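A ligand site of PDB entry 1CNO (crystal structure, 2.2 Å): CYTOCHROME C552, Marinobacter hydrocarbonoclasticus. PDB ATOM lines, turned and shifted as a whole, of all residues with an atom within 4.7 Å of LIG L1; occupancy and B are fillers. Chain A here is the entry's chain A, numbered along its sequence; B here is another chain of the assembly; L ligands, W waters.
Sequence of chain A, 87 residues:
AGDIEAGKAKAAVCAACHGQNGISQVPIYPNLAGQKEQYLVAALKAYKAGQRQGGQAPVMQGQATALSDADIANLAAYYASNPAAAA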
ATOM      1  N   VAL A  13      32.461 -10.642  -8.888  1.00  0.00           N
ATOM      2  CA  VAL A  13      33.616  -9.986  -9.509  1.00  0.00           C
ATOM      3  C   VAL A  13      33.204  -9.213 -10.794  1.00  0.00           C
ATOM      4  O   VAL A  13      34.009  -8.492 -11.388  1.00  0.00           O
ATOM      5  CB  VAL A  13      34.740 -11.011  -9.818  1.00  0.00           C
ATOM      6  CG1 VAL A  13      34.346 -11.926 -10.972  1.00  0.00           C
ATOM      7  CG2 VAL A  13      36.039 -10.299 -10.109  1.00  0.00           C
ATOM      8  N   CYS A  14      31.924  -9.324 -11.142  1.00  0.00           N
ATOM      9  CA  CYS A  14      31.333  -8.689 -12.326  1.00  0.00           C
ATOM     10  C   CYS A  14      30.535  -7.423 -11.968  1.00  0.00           C
ATOM     11  O   CYS A  14      30.550  -6.412 -12.711  1.00  0.00           O
ATOM     12  CB  CYS A  14      30.380  -9.690 -12.996  1.00  0.00           C
ATOM     13  SG  CYS A  14      31.128 -11.281 -13.364  1.00  0.00           S
ATOM     14  N   CYS A  17      31.161  -3.454 -12.293  1.00  0.00           N
ATOM     15  CA  CYS A  17      30.990  -2.807 -13.588  1.00  0.00           C
ATOM     16  C   CYS A  17      29.606  -2.952 -14.214  1.00  0.00           C
ATOM     17  O   CYS A  17      29.053  -1.996 -14.729  1.00  0.00           O
ATOM     18  CB  CYS A  17      32.004  -3.367 -14.553  1.00  0.00           C
ATOM     19  SG  CYS A  17      33.717  -2.893 -14.235  1.00  0.00           S
ATOM     20  N   HIS A  18      29.061  -4.164 -14.150  1.00  0.00           N
ATOM     21  CA  HIS A  18      27.758  -4.465 -14.731  1.00  0.00           C
ATOM     22  C   HIS A  18      26.563  -4.280 -13.788  1.00  0.00           C
ATOM     23  O   HIS A  18      25.420  -4.523 -14.172  1.00  0.00           O
ATOM     24  CB  HIS A  18      27.770  -5.878 -15.320  1.00  0.00           C
ATOM     25  CG  HIS A  18      28.718  -6.031 -16.500  1.00  0.00           C
ATOM     26  ND1 HIS A  18      28.486  -5.402 -17.728  1.00  0.00           N
ATOM     27  CD2 HIS A  18      29.873  -6.667 -16.614  1.00  0.00           C
ATOM     28  CE1 HIS A  18      29.526  -5.711 -18.515  1.00  0.00           C
ATOM     29  NE2 HIS A  18      30.396  -6.474 -17.897  1.00  0.00           N
ATOM     30  N   ILE A  28      29.267   3.126 -20.665  1.00  0.00           N
ATOM     31  CA  ILE A  28      30.041   2.392 -21.653  1.00  0.00           C
ATOM     32  C   ILE A  28      30.102   0.919 -21.276  1.00  0.00           C
ATOM     33  O   ILE A  28      30.695   0.102 -21.986  1.00  0.00           O
ATOM     34  CB  ILE A  28      31.468   2.983 -21.844  1.00  0.00           C
ATOM     35  CG1 ILE A  28      32.292   2.823 -20.547  1.00  0.00           C
ATOM     36  CG2 ILE A  28      31.368   4.458 -22.272  1.00  0.00           C
ATOM     37  CD1 ILE A  28      33.773   3.126 -20.708  1.00  0.00           C
ATOM     38  N   TYR A  29      29.532   0.586 -20.109  1.00  0.00           N
ATOM     39  CA  TYR A  29      29.488  -0.801 -19.662  1.00  0.00           C
ATOM     40  C   TYR A  29      28.063  -1.266 -19.963  1.00  0.00           C
ATOM     41  O   TYR A  29      27.084  -0.645 -19.526  1.00  0.00           O
ATOM     42  CB  TYR A  29      29.748  -0.936 -18.161  1.00  0.00           C
ATOM     43  CG  TYR A  29      31.139  -0.574 -17.685  1.00  0.00           C
ATOM     44  CD1 TYR A  29      32.208  -0.487 -18.569  1.00  0.00           C
ATOM     45  CD2 TYR A  29      31.398  -0.354 -16.321  1.00  0.00           C
ATOM     46  CE1 TYR A  29      33.487  -0.182 -18.129  1.00  0.00           C
ATOM     47  CE2 TYR A  29      32.681  -0.054 -15.869  1.00  0.00           C
ATOM     48  CZ  TYR A  29      33.719   0.025 -16.779  1.00  0.00           C
ATOM     49  OH  TYR A  29      34.982   0.298 -16.340  1.00  0.00           O
ATOM     50  N   PRO A  30      27.914  -2.342 -20.758  1.00  0.00           N
ATOM     51  CA  PRO A  30      26.591  -2.854 -21.103  1.00  0.00           C
ATOM     52  C   PRO A  30      25.769  -3.518 -19.990  1.00  0.00           C
ATOM     53  O   PRO A  30      26.321  -4.064 -19.013  1.00  0.00           O
ATOM     54  CB  PRO A  30      26.891  -3.852 -22.230  1.00  0.00           C
ATOM     55  CG  PRO A  30      28.271  -4.340 -21.928  1.00  0.00           C
ATOM     56  CD  PRO A  30      28.981  -3.076 -21.478  1.00  0.00           C
ATOM     57  N   LEU A  32      23.474  -6.442 -18.648  1.00  0.00           N
ATOM     58  CA  LEU A  32      23.445  -7.881 -18.891  1.00  0.00           C
ATOM     59  C   LEU A  32      22.121  -8.544 -18.484  1.00  0.00           C
ATOM     60  O   LEU A  32      21.783  -9.605 -18.997  1.00  0.00           O
ATOM     61  CB  LEU A  32      24.602  -8.567 -18.139  1.00  0.00           C
ATOM     62  CG  LEU A  32      26.050  -8.078 -18.355  1.00  0.00           C
ATOM     63  CD1 LEU A  32      27.034  -9.024 -17.627  1.00  0.00           C
ATOM     64  CD2 LEU A  32      26.387  -8.004 -19.870  1.00  0.00           C
ATOM     65  N   TYR A  39      23.383 -16.026 -26.113  1.00  0.00           N
ATOM     66  CA  TYR A  39      24.184 -14.913 -26.580  1.00  0.00           C
ATOM     67  C   TYR A  39      25.229 -14.535 -25.532  1.00  0.00           C
ATOM     68  O   TYR A  39      26.372 -14.219 -25.894  1.00  0.00           O
ATOM     69  CB  TYR A  39      23.305 -13.689 -26.870  1.00  0.00           C
ATOM     70  CG  TYR A  39      24.142 -12.489 -27.215  1.00  0.00           C
ATOM     71  CD1 TYR A  39      24.848 -12.431 -28.421  1.00  0.00           C
ATOM     72  CD2 TYR A  39      24.278 -11.429 -26.311  1.00  0.00           C
ATOM     73  CE1 TYR A  39      25.698 -11.364 -28.707  1.00  0.00           C
ATOM     74  CE2 TYR A  39      25.115 -10.360 -26.576  1.00  0.00           C
ATOM     75  CZ  TYR A  39      25.819 -10.334 -27.779  1.00  0.00           C
ATOM     76  OH  TYR A  39      26.659  -9.288 -28.062  1.00  0.00           O
ATOM     77  N   LEU A  40      24.818 -14.523 -24.262  1.00  0.00           N
ATOM     78  CA  LEU A  40      25.726 -14.193 -23.143  1.00  0.00           C
ATOM     79  C   LEU A  40      26.925 -15.156 -23.138  1.00  0.00           C
ATOM     80  O   LEU A  40      28.059 -14.732 -22.971  1.00  0.00           O
ATOM     81  CB  LEU A  40      24.980 -14.232 -21.796  1.00  0.00           C
ATOM     82  CG  LEU A  40      24.064 -13.050 -21.485  1.00  0.00           C
ATOM     83  CD1 LEU A  40      23.274 -13.246 -20.184  1.00  0.00           C
ATOM     84  CD2 LEU A  40      24.872 -11.780 -21.415  1.00  0.00           C
ATOM     85  N   ALA A  43      29.121 -14.266 -26.283  1.00  0.00           N
ATOM     86  CA  ALA A  43      29.876 -13.032 -26.092  1.00  0.00           C
ATOM     87  C   ALA A  43      31.091 -13.271 -25.176  1.00  0.00           C
ATOM     88  O   ALA A  43      32.217 -12.859 -25.499  1.00  0.00           O
ATOM     89  CB  ALA A  43      28.974 -11.917 -25.526  1.00  0.00           C
ATOM     90  N   LEU A  44      30.863 -13.974 -24.059  1.00  0.00           N
ATOM     91  CA  LEU A  44      31.925 -14.286 -23.102  1.00  0.00           C
ATOM     92  C   LEU A  44      33.031 -15.145 -23.720  1.00  0.00           C
ATOM     93  O   LEU A  44      34.218 -14.851 -23.537  1.00  0.00           O
ATOM     94  CB  LEU A  44      31.366 -14.955 -21.843  1.00  0.00           C
ATOM     95  CG  LEU A  44      30.684 -13.980 -20.893  1.00  0.00           C
ATOM     96  CD1 LEU A  44      29.929 -14.747 -19.814  1.00  0.00           C
ATOM     97  CD2 LEU A  44      31.737 -13.013 -20.285  1.00  0.00           C
ATOM     98  N   TYR A  47      35.180 -12.836 -25.975  1.00  0.00           N
ATOM     99  CA  TYR A  47      36.153 -12.042 -25.207  1.00  0.00           C
ATOM    100  C   TYR A  47      37.296 -12.930 -24.729  1.00  0.00           C
ATOM    101  O   TYR A  47      38.453 -12.553 -24.797  1.00  0.00           O
ATOM    102  CB  TYR A  47      35.505 -11.391 -23.974  1.00  0.00           C
ATOM    103  CG  TYR A  47      34.587 -10.243 -24.308  1.00  0.00           C
ATOM    104  CD1 TYR A  47      35.084  -9.073 -24.887  1.00  0.00           C
ATOM    105  CD2 TYR A  47      33.207 -10.333 -24.048  1.00  0.00           C
ATOM    106  CE1 TYR A  47      34.227  -7.997 -25.224  1.00  0.00           C
ATOM    107  CE2 TYR A  47      32.344  -9.260 -24.393  1.00  0.00           C
ATOM    108  CZ  TYR A  47      32.862  -8.120 -24.974  1.00  0.00           C
ATOM    109  OH  TYR A  47      32.013  -7.104 -25.331  1.00  0.00           O
ATOM    110  N   ARG A  52      36.934 -10.048 -29.733  1.00  0.00           N
ATOM    111  CA  ARG A  52      36.327  -8.708 -29.788  1.00  0.00           C
ATOM    112  C   ARG A  52      37.419  -7.664 -29.600  1.00  0.00           C
ATOM    113  O   ARG A  52      38.190  -7.692 -28.622  1.00  0.00           O
ATOM    114  CB  ARG A  52      35.196  -8.542 -28.753  1.00  0.00           C
ATOM    115  CG  ARG A  52      33.971  -9.400 -29.092  1.00  0.00           C
ATOM    116  CD  ARG A  52      32.760  -9.052 -28.219  1.00  0.00           C
ATOM    117  NE  ARG A  52      31.552  -9.682 -28.747  1.00  0.00           N
ATOM    118  CZ  ARG A  52      30.336  -9.554 -28.253  1.00  0.00           C
ATOM    119  NH1 ARG A  52      30.121  -8.785 -27.186  1.00  0.00           N
ATOM    120  NH2 ARG A  52      29.314 -10.136 -28.875  1.00  0.00           N
ATOM    121  N   GLN A  56      36.338  -0.383 -25.817  1.00  0.00           N
ATOM    122  CA  GLN A  56      36.650  -0.904 -24.497  1.00  0.00           C
ATOM    123  C   GLN A  56      36.699  -2.430 -24.418  1.00  0.00           C
ATOM    124  O   GLN A  56      36.777  -2.983 -23.317  1.00  0.00           O
ATOM    125  CB  GLN A  56      35.638  -0.348 -23.478  1.00  0.00           C
ATOM    126  CG  GLN A  56      35.692   1.178 -23.318  1.00  0.00           C
ATOM    127  CD  GLN A  56      37.013   1.679 -22.688  1.00  0.00           C
ATOM    128  OE1 GLN A  56      37.794   0.900 -22.130  1.00  0.00           O
ATOM    129  NE2 GLN A  56      37.239   2.986 -22.764  1.00  0.00           N
ATOM    130  N   ALA A  57      36.677  -3.115 -25.566  1.00  0.00           N
ATOM    131  CA  ALA A  57      36.756  -4.584 -25.600  1.00  0.00           C
ATOM    132  C   ALA A  57      37.984  -5.125 -24.857  1.00  0.00           C
ATOM    133  O   ALA A  57      37.876  -6.131 -24.179  1.00  0.00           O
ATOM    134  CB  ALA A  57      36.718  -5.119 -27.064  1.00  0.00           C
ATOM    135  N   VAL A  59      39.315  -4.133 -22.262  1.00  0.00           N
ATOM    136  CA  VAL A  59      38.995  -4.139 -20.828  1.00  0.00           C
ATOM    137  C   VAL A  59      38.196  -5.414 -20.478  1.00  0.00           C
ATOM    138  O   VAL A  59      38.532  -6.132 -19.529  1.00  0.00           O
ATOM    139  CB  VAL A  59      38.198  -2.845 -20.402  1.00  0.00           C
ATOM    140  CG1 VAL A  59      37.537  -3.038 -19.028  1.00  0.00           C
ATOM    141  CG2 VAL A  59      39.132  -1.619 -20.382  1.00  0.00           C
ATOM    142  N   MET A  60      37.162  -5.719 -21.275  1.00  0.00           N
ATOM    143  CA  MET A  60      36.371  -6.924 -21.002  1.00  0.00           C
ATOM    144  C   MET A  60      37.145  -8.200 -21.325  1.00  0.00           C
ATOM    145  O   MET A  60      36.951  -9.250 -20.694  1.00  0.00           O
ATOM    146  CB  MET A  60      35.027  -6.904 -21.714  1.00  0.00           C
ATOM    147  CG  MET A  60      34.135  -8.106 -21.353  1.00  0.00           C
ATOM    148  SD  MET A  60      33.849  -8.274 -19.558  1.00  0.00           S
ATOM    149  CE  MET A  60      33.924 -10.053 -19.419  1.00  0.00           C
ATOM    150  N   GLN A  63      38.838  -9.352 -18.307  1.00  0.00           N
ATOM    151  CA  GLN A  63      37.972  -9.948 -17.296  1.00  0.00           C
ATOM    152  C   GLN A  63      37.453 -11.335 -17.667  1.00  0.00           C
ATOM    153  O   GLN A  63      36.944 -12.063 -16.817  1.00  0.00           O
ATOM    154  CB  GLN A  63      36.775  -9.016 -17.011  1.00  0.00           C
ATOM    155  CG  GLN A  63      37.134  -7.582 -16.658  1.00  0.00           C
ATOM    156  CD  GLN A  63      37.905  -7.460 -15.361  1.00  0.00           C
ATOM    157  OE1 GLN A  63      37.682  -8.208 -14.401  1.00  0.00           O
ATOM    158  NE2 GLN A  63      38.822  -6.486 -15.315  1.00  0.00           N
ATOM    159  N   LEU A  67      38.060 -17.050 -16.913  1.00  0.00           N
ATOM    160  CA  LEU A  67      36.802 -17.772 -16.769  1.00  0.00           C
ATOM    161  C   LEU A  67      36.834 -19.139 -17.433  1.00  0.00           C
ATOM    162  O   LEU A  67      37.273 -19.273 -18.580  1.00  0.00           O
ATOM    163  CB  LEU A  67      35.649 -16.959 -17.380  1.00  0.00           C
ATOM    164  CG  LEU A  67      35.326 -15.580 -16.780  1.00  0.00           C
ATOM    165  CD1 LEU A  67      34.194 -14.923 -17.551  1.00  0.00           C
ATOM    166  CD2 LEU A  67      34.968 -15.720 -15.286  1.00  0.00           C
ATOM    167  N   LEU A  75      27.418 -17.953 -15.387  1.00  0.00           N
ATOM    168  CA  LEU A  75      27.222 -16.506 -15.454  1.00  0.00           C
ATOM    169  C   LEU A  75      26.107 -16.143 -16.444  1.00  0.00           C
ATOM    170  O   LEU A  75      25.235 -15.342 -16.124  1.00  0.00           O
ATOM    171  CB  LEU A  75      28.544 -15.786 -15.804  1.00  0.00           C
ATOM    172  CG  LEU A  75      29.585 -15.870 -14.663  1.00  0.00           C
ATOM    173  CD1 LEU A  75      31.002 -15.481 -15.144  1.00  0.00           C
ATOM    174  CD2 LEU A  75      29.142 -14.973 -13.518  1.00  0.00           C
ATOM    175  N   TYR A  79      22.702 -14.116 -15.286  1.00  0.00           N
ATOM    176  CA  TYR A  79      22.317 -12.837 -15.892  1.00  0.00           C
ATOM    177  C   TYR A  79      21.053 -12.918 -16.729  1.00  0.00           C
ATOM    178  O   TYR A  79      20.201 -12.047 -16.626  1.00  0.00           O
ATOM    179  CB  TYR A  79      23.480 -12.234 -16.682  1.00  0.00           C
ATOM    180  CG  TYR A  79      24.525 -11.610 -15.777  1.00  0.00           C
ATOM    181  CD1 TYR A  79      24.194 -10.495 -15.007  1.00  0.00           C
ATOM    182  CD2 TYR A  79      25.828 -12.131 -15.681  1.00  0.00           C
ATOM    183  CE1 TYR A  79      25.108  -9.914 -14.143  1.00  0.00           C
ATOM    184  CE2 TYR A  79      26.769 -11.536 -14.804  1.00  0.00           C
ATOM    185  CZ  TYR A  79      26.387 -10.439 -14.041  1.00  0.00           C
ATOM    186  OH  TYR A  79      27.249  -9.844 -13.172  1.00  0.00           O
ATOM    187  N   GLN B  35      19.388  -0.906 -23.999  1.00  0.00           N
ATOM    188  CA  GLN B  35      20.813  -1.099 -23.737  1.00  0.00           C
ATOM    189  C   GLN B  35      21.432   0.305 -23.687  1.00  0.00           C
ATOM    190  O   GLN B  35      20.860   1.250 -24.249  1.00  0.00           O
ATOM    191  CB  GLN B  35      21.447  -1.949 -24.874  1.00  0.00           C
ATOM    192  CG  GLN B  35      22.946  -2.213 -24.731  1.00  0.00           C
ATOM    193  CD  GLN B  35      23.311  -2.881 -23.402  1.00  0.00           C
ATOM    194  OE1 GLN B  35      23.659  -2.187 -22.424  1.00  0.00           O
ATOM    195  NE2 GLN B  35      23.211  -4.214 -23.346  1.00  0.00           N
ATOM    196  N   TYR B  39      27.229   2.322 -25.438  1.00  0.00           N
ATOM    197  CA  TYR B  39      27.714   0.984 -25.728  1.00  0.00           C
ATOM    198  C   TYR B  39      27.189   0.474 -27.100  1.00  0.00           C
ATOM    199  O   TYR B  39      27.934  -0.181 -27.821  1.00  0.00           O
ATOM    200  CB  TYR B  39      27.353  -0.006 -24.627  1.00  0.00           C
ATOM    201  CG  TYR B  39      27.651  -1.433 -25.017  1.00  0.00           C
ATOM    202  CD1 TYR B  39      28.972  -1.912 -25.044  1.00  0.00           C
ATOM    203  CD2 TYR B  39      26.635  -2.286 -25.436  1.00  0.00           C
ATOM    204  CE1 TYR B  39      29.275  -3.213 -25.477  1.00  0.00           C
ATOM    205  CE2 TYR B  39      26.922  -3.595 -25.867  1.00  0.00           C
ATOM    206  CZ  TYR B  39      28.252  -4.038 -25.890  1.00  0.00           C
ATOM    207  OH  TYR B  39      28.552  -5.286 -26.356  1.00  0.00           O
ATOM    208  N   ARG B  52      34.734  -7.441 -34.596  1.00  0.00           N
ATOM    209  CA  ARG B  52      34.087  -8.503 -33.844  1.00  0.00           C
ATOM    210  C   ARG B  52      34.058  -9.789 -34.654  1.00  0.00           C
ATOM    211  O   ARG B  52      33.542  -9.823 -35.770  1.00  0.00           O
ATOM    212  CB  ARG B  52      32.687  -8.096 -33.381  1.00  0.00           C
ATOM    213  CG  ARG B  52      32.692  -7.158 -32.208  1.00  0.00           C
ATOM    214  CD  ARG B  52      31.315  -6.999 -31.579  1.00  0.00           C
ATOM    215  NE  ARG B  52      31.391  -6.244 -30.329  1.00  0.00           N
ATOM    216  CZ  ARG B  52      30.393  -6.061 -29.481  1.00  0.00           C
ATOM    217  NH1 ARG B  52      29.194  -6.576 -29.707  1.00  0.00           N
ATOM    218  NH2 ARG B  52      30.620  -5.380 -28.367  1.00  0.00           N
HETATM  219 FE1  LIG L   1      31.973  -7.280 -18.761  1.00  0.00          FE
HETATM  220  C1  LIG L   1      31.033  -6.443 -21.909  1.00  0.00           C
HETATM  221  C2  LIG L   1      30.052 -10.082 -18.956  1.00  0.00           C
HETATM  222  C3  LIG L   1      33.175  -8.237 -15.706  1.00  0.00           C
HETATM  223  C4  LIG L   1      33.494  -4.266 -18.445  1.00  0.00           C
HETATM  224  N1  LIG L   1      30.836  -8.132 -20.173  1.00  0.00           N
HETATM  225  C5  LIG L   1      30.594  -7.661 -21.432  1.00  0.00           C
HETATM  226  C6  LIG L   1      29.713  -8.564 -22.131  1.00  0.00           C
HETATM  227  C7  LIG L   1      29.410  -9.619 -21.325  1.00  0.00           C
HETATM  228  C8  LIG L   1      30.084  -9.295 -20.079  1.00  0.00           C
HETATM  229  C9  LIG L   1      28.545 -10.872 -21.610  1.00  0.00           C
HETATM  230  C10 LIG L   1      29.208  -8.317 -23.547  1.00  0.00           C
HETATM  231  C11 LIG L   1      27.766  -7.900 -23.428  1.00  0.00           C
HETATM  232  C12 LIG L   1      27.084  -7.657 -24.774  1.00  0.00           C
HETATM  233  O1  LIG L   1      26.051  -6.950 -24.756  1.00  0.00           O
HETATM  234  O2  LIG L   1      27.567  -8.151 -25.816  1.00  0.00           O
HETATM  235  N2  LIG L   1      31.679  -8.834 -17.617  1.00  0.00           N
HETATM  236  C13 LIG L   1      30.827  -9.895 -17.808  1.00  0.00           C
HETATM  237  C14 LIG L   1      30.951 -10.885 -16.756  1.00  0.00           C
HETATM  238  C15 LIG L   1      31.941 -10.426 -15.913  1.00  0.00           C
HETATM  239  C16 LIG L   1      32.371  -9.143 -16.422  1.00  0.00           C
HETATM  240  C17 LIG L   1      30.070 -12.116 -16.603  1.00  0.00           C
HETATM  241  C18 LIG L   1      32.463 -11.026 -14.612  1.00  0.00           C
HETATM  242  C19 LIG L   1      33.033 -12.411 -14.629  1.00  0.00           C
HETATM  243  N3  LIG L   1      33.039  -6.399 -17.345  1.00  0.00           N
HETATM  244  C20 LIG L   1      33.440  -6.929 -16.129  1.00  0.00           C
HETATM  245  C21 LIG L   1      34.165  -5.941 -15.361  1.00  0.00           C
HETATM  246  C22 LIG L   1      34.236  -4.818 -16.153  1.00  0.00           C
HETATM  247  C23 LIG L   1      33.562  -5.133 -17.363  1.00  0.00           C
HETATM  248  C24 LIG L   1      34.596  -6.160 -13.902  1.00  0.00           C
HETATM  249  C25 LIG L   1      34.650  -3.433 -15.743  1.00  0.00           C
HETATM  250  C26 LIG L   1      36.072  -3.175 -15.272  1.00  0.00           C
HETATM  251  N4  LIG L   1      32.282  -5.752 -19.944  1.00  0.00           N
HETATM  252  C27 LIG L   1      32.941  -4.553 -19.665  1.00  0.00           C
HETATM  253  C28 LIG L   1      33.001  -3.674 -20.823  1.00  0.00           C
HETATM  254  C29 LIG L   1      32.276  -4.262 -21.772  1.00  0.00           C
HETATM  255  C30 LIG L   1      31.825  -5.537 -21.237  1.00  0.00           C
HETATM  256  C31 LIG L   1      34.025  -2.549 -21.026  1.00  0.00           C
HETATM  257  C32 LIG L   1      32.138  -3.812 -23.233  1.00  0.00           C
HETATM  258  C33 LIG L   1      33.206  -4.451 -24.113  1.00  0.00           C
HETATM  259  C34 LIG L   1      33.053  -4.087 -25.567  1.00  0.00           C
HETATM  260  O3  LIG L   1      32.953  -2.889 -25.865  1.00  0.00           O
HETATM  261  O4  LIG L   1      32.999  -5.002 -26.435  1.00  0.00           O
HETATM  262 FE1  LG2 L   2      22.471  -7.192 -35.069  1.00  0.00          FE
HETATM  263  C1  LG2 L   2      24.583  -8.173 -32.599  1.00  0.00           C
HETATM  264  C2  LG2 L   2      22.553  -3.971 -33.939  1.00  0.00           C
HETATM  265  C3  LG2 L   2      20.708  -6.163 -37.796  1.00  0.00           C
HETATM  266  C4  LG2 L   2      22.083 -10.446 -36.019  1.00  0.00           C
HETATM  267  N1  LG2 L   2      23.311  -6.269 -33.580  1.00  0.00           N
HETATM  268  C5  LG2 L   2      24.139  -6.854 -32.610  1.00  0.00           C
HETATM  269  C6  LG2 L   2      24.586  -5.845 -31.681  1.00  0.00           C
HETATM  270  C7  LG2 L   2      24.073  -4.642 -32.080  1.00  0.00           C
HETATM  271  C8  LG2 L   2      23.265  -4.927 -33.267  1.00  0.00           C
HETATM  272  C9  LG2 L   2      24.240  -3.271 -31.397  1.00  0.00           C
HETATM  273  C10 LG2 L   2      25.429  -6.086 -30.457  1.00  0.00           C
HETATM  274  C11 LG2 L   2      24.548  -6.372 -29.261  1.00  0.00           C
HETATM  275  C12 LG2 L   2      25.335  -6.472 -27.975  1.00  0.00           C
HETATM  276  O1  LG2 L   2      24.707  -6.657 -26.920  1.00  0.00           O
HETATM  277  O2  LG2 L   2      26.580  -6.350 -28.028  1.00  0.00           O
HETATM  278  N2  LG2 L   2      21.788  -5.438 -35.691  1.00  0.00           N
HETATM  279  C13 LG2 L   2      21.870  -4.215 -35.093  1.00  0.00           C
HETATM  280  C14 LG2 L   2      21.269  -3.188 -35.906  1.00  0.00           C
HETATM  281  C15 LG2 L   2      20.860  -3.795 -37.060  1.00  0.00           C
HETATM  282  C16 LG2 L   2      21.122  -5.196 -36.890  1.00  0.00           C
HETATM  283  C17 LG2 L   2      21.022  -1.754 -35.427  1.00  0.00           C
HETATM  284  C18 LG2 L   2      20.113  -3.157 -38.233  1.00  0.00           C
HETATM  285  C19 LG2 L   2      20.731  -1.924 -38.903  1.00  0.00           C
HETATM  286  N3  LG2 L   2      21.594  -8.111 -36.584  1.00  0.00           N
HETATM  287  C20 LG2 L   2      20.908  -7.510 -37.656  1.00  0.00           C
HETATM  288  C21 LG2 L   2      20.267  -8.499 -38.499  1.00  0.00           C
HETATM  289  C22 LG2 L   2      20.618  -9.719 -37.944  1.00  0.00           C
HETATM  290  C23 LG2 L   2      21.443  -9.458 -36.773  1.00  0.00           C
HETATM  291  C24 LG2 L   2      19.287  -8.196 -39.645  1.00  0.00           C
HETATM  292  C25 LG2 L   2      20.100 -11.097 -38.320  1.00  0.00           C
HETATM  293  C26 LG2 L   2      20.233 -11.679 -39.721  1.00  0.00           C
HETATM  294  N4  LG2 L   2      23.250  -8.941 -34.482  1.00  0.00           N
HETATM  295  C27 LG2 L   2      22.952 -10.226 -34.983  1.00  0.00           C
HETATM  296  C28 LG2 L   2      23.766 -11.229 -34.354  1.00  0.00           C
HETATM  297  C29 LG2 L   2      24.464 -10.574 -33.359  1.00  0.00           C
HETATM  298  C30 LG2 L   2      24.154  -9.161 -33.444  1.00  0.00           C
HETATM  299  C31 LG2 L   2      23.942 -12.695 -34.793  1.00  0.00           C
HETATM  300  C32 LG2 L   2      25.465 -11.224 -32.398  1.00  0.00           C
HETATM  301  C33 LG2 L   2      26.822 -11.222 -33.081  1.00  0.00           C
HETATM  302  C34 LG2 L   2      27.959 -11.567 -32.114  1.00  0.00           C
HETATM  303  O3  LG2 L   2      27.971 -12.712 -31.612  1.00  0.00           O
HETATM  304  O4  LG2 L   2      28.820 -10.696 -31.862  1.00  0.00           O
HETATM  305  O   HOH W   1      34.024  -5.135 -29.679  1.00  0.00           O
HETATM  306  O   HOH W   2      35.608  -9.665 -13.647  1.00  0.00           O
HETATM  307  O   HOH W   3      33.001  -2.934 -28.620  1.00  0.00           O
HETATM  308  O   HOH W   4      33.389  -0.156 -26.000  1.00  0.00           O
HETATM  309  O   HOH W   5      23.784  -7.568 -23.009  1.00  0.00           O
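Residues that only touch LIG L1: Val 13 (3.5 Å), Tyr 29 (3.7 Å), Pro 30 (3.5 Å), Leu 32 (3.5 Å), Leu 40 (3.8 Å), Leu 44 (3.6 Å), Gln 56 (3.6 Å), Ala 57 (3.7 Å), Gln 63 (3.6 Å), Leu 67 (3.9 Å), Leu 75 (3.7 Å) and Tyr 79 (3.8 Å).
Hydrophobic or aromatic side chains within 4 Å of LIG L1: Val 13, His 18, Tyr 29, Pro 30, Leu 32, Tyr 39 of chain A, Leu 40, Leu 44, Tyr 47, Ala 57, Met 60, Leu 67, Leu 75, Tyr 79 and Tyr 39 of chain B.
Of the 25 residues printed, 21 come within 4 Å of LIG L1.
Along chain A the residues within 4 Å of LIG L1 span positions 13 to 79.
Water W3 bridges O3 of LIG L1 (2.8 Å) and NH2 of Arg 52 of chain B (3.4 Å).
Water W4 lies within hydrogen-bond range of an oxygen (O3) of LIG L1 (2.8 Å) and the backbone NH of Gln 56 (3.0 Å).
Water W5 lies within hydrogen-bond range of an oxygen (O1) of LIG L1 (2.9 Å) and the side-chain amide nitrogen of Gln 35 of chain B (3.4 Å).
Water W1 lies within hydrogen-bond range of NE of Arg 52 of chain B (2.9 Å) and O4 of LIG L1 (3.4 Å).
Water W2 lies within hydrogen-bond range of the side-chain amide oxygen (OE1) of Gln 63 (2.6 Å) and the backbone carbonyl oxygen (O) of Val 13 (3.0 Å).
An oxygen (O1) of LG2 L2 lies close to an oxygen (O1) of LIG L1, at 2.6 Å.
A carbon (C18) of LIG L1 is bonded to the side-chain sulfur (SG) of Cys 14 (1.8 Å).
SG of Cys 17 is bonded to C25 of LIG L1, at 1.9 Å.
An iron atom (FE1) of LIG L1 is bound by a ring nitrogen (NE2) of His 18 (2.0 Å).
The side-chain sulfur (SD) of Met 60 is bound to an iron atom (FE1) of LIG L1 (2.3 Å).
OH of Tyr 47 is in hydrogen-bond range of O4 of LIG L1 (2.6 Å).
The side-chain hydroxyl (OH) of Tyr 39 of chain A is in hydrogen-bond range of an oxygen (O2) of LIG L1.
NH1 of Arg 52 of chain A is in salt-bridge range of O2 of LIG L1 (3.0 Å).
OH of Tyr 39 of chain B is in hydrogen-bond range of O2 of LIG L1, 3.1 Å away.
An oxygen (O4) of LIG L1 is in salt-bridge range of the guanidinium group (NH2) of Arg 52 of chain B, at 3.1 Å.
An oxygen (O2) of LG2 L2 sits at hydrogen-bond distance from the side-chain hydroxyl of Tyr 39 of chain A (2.9 Å).
The guanidinium group (NH2) of Arg 52 of chain A is in salt-bridge range of an oxygen (O4) of LG2 L2.
An oxygen (O2) of LG2 L2 lies within hydrogen-bond range of the side-chain hydroxyl of Tyr 39 of chain B, 2.8 Å away.
NH1 of Arg 52 of chain B lies within salt-bridge range of O2 of LG2 L2 (3.1 Å).
The backbone carbonyl oxygen (O) of Pro 30 sits at hydrogen-bond distance from a ring nitrogen (ND1) of His 18 (2.9 Å).
OH of Tyr 47 lies within hydrogen-bond range of NH1 of Arg 52 of chain A, at 3.1 Å.
The guanidinium group of Arg 52 of chain A sits at hydrogen-bond distance from the side-chain hydroxyl of Tyr 39 of chain A (2.9 Å).
The guanidinium group (NH2) of Arg 52 of chain B is in hydrogen-bond range of the side-chain hydroxyl (OH) of Tyr 39 of chain B.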
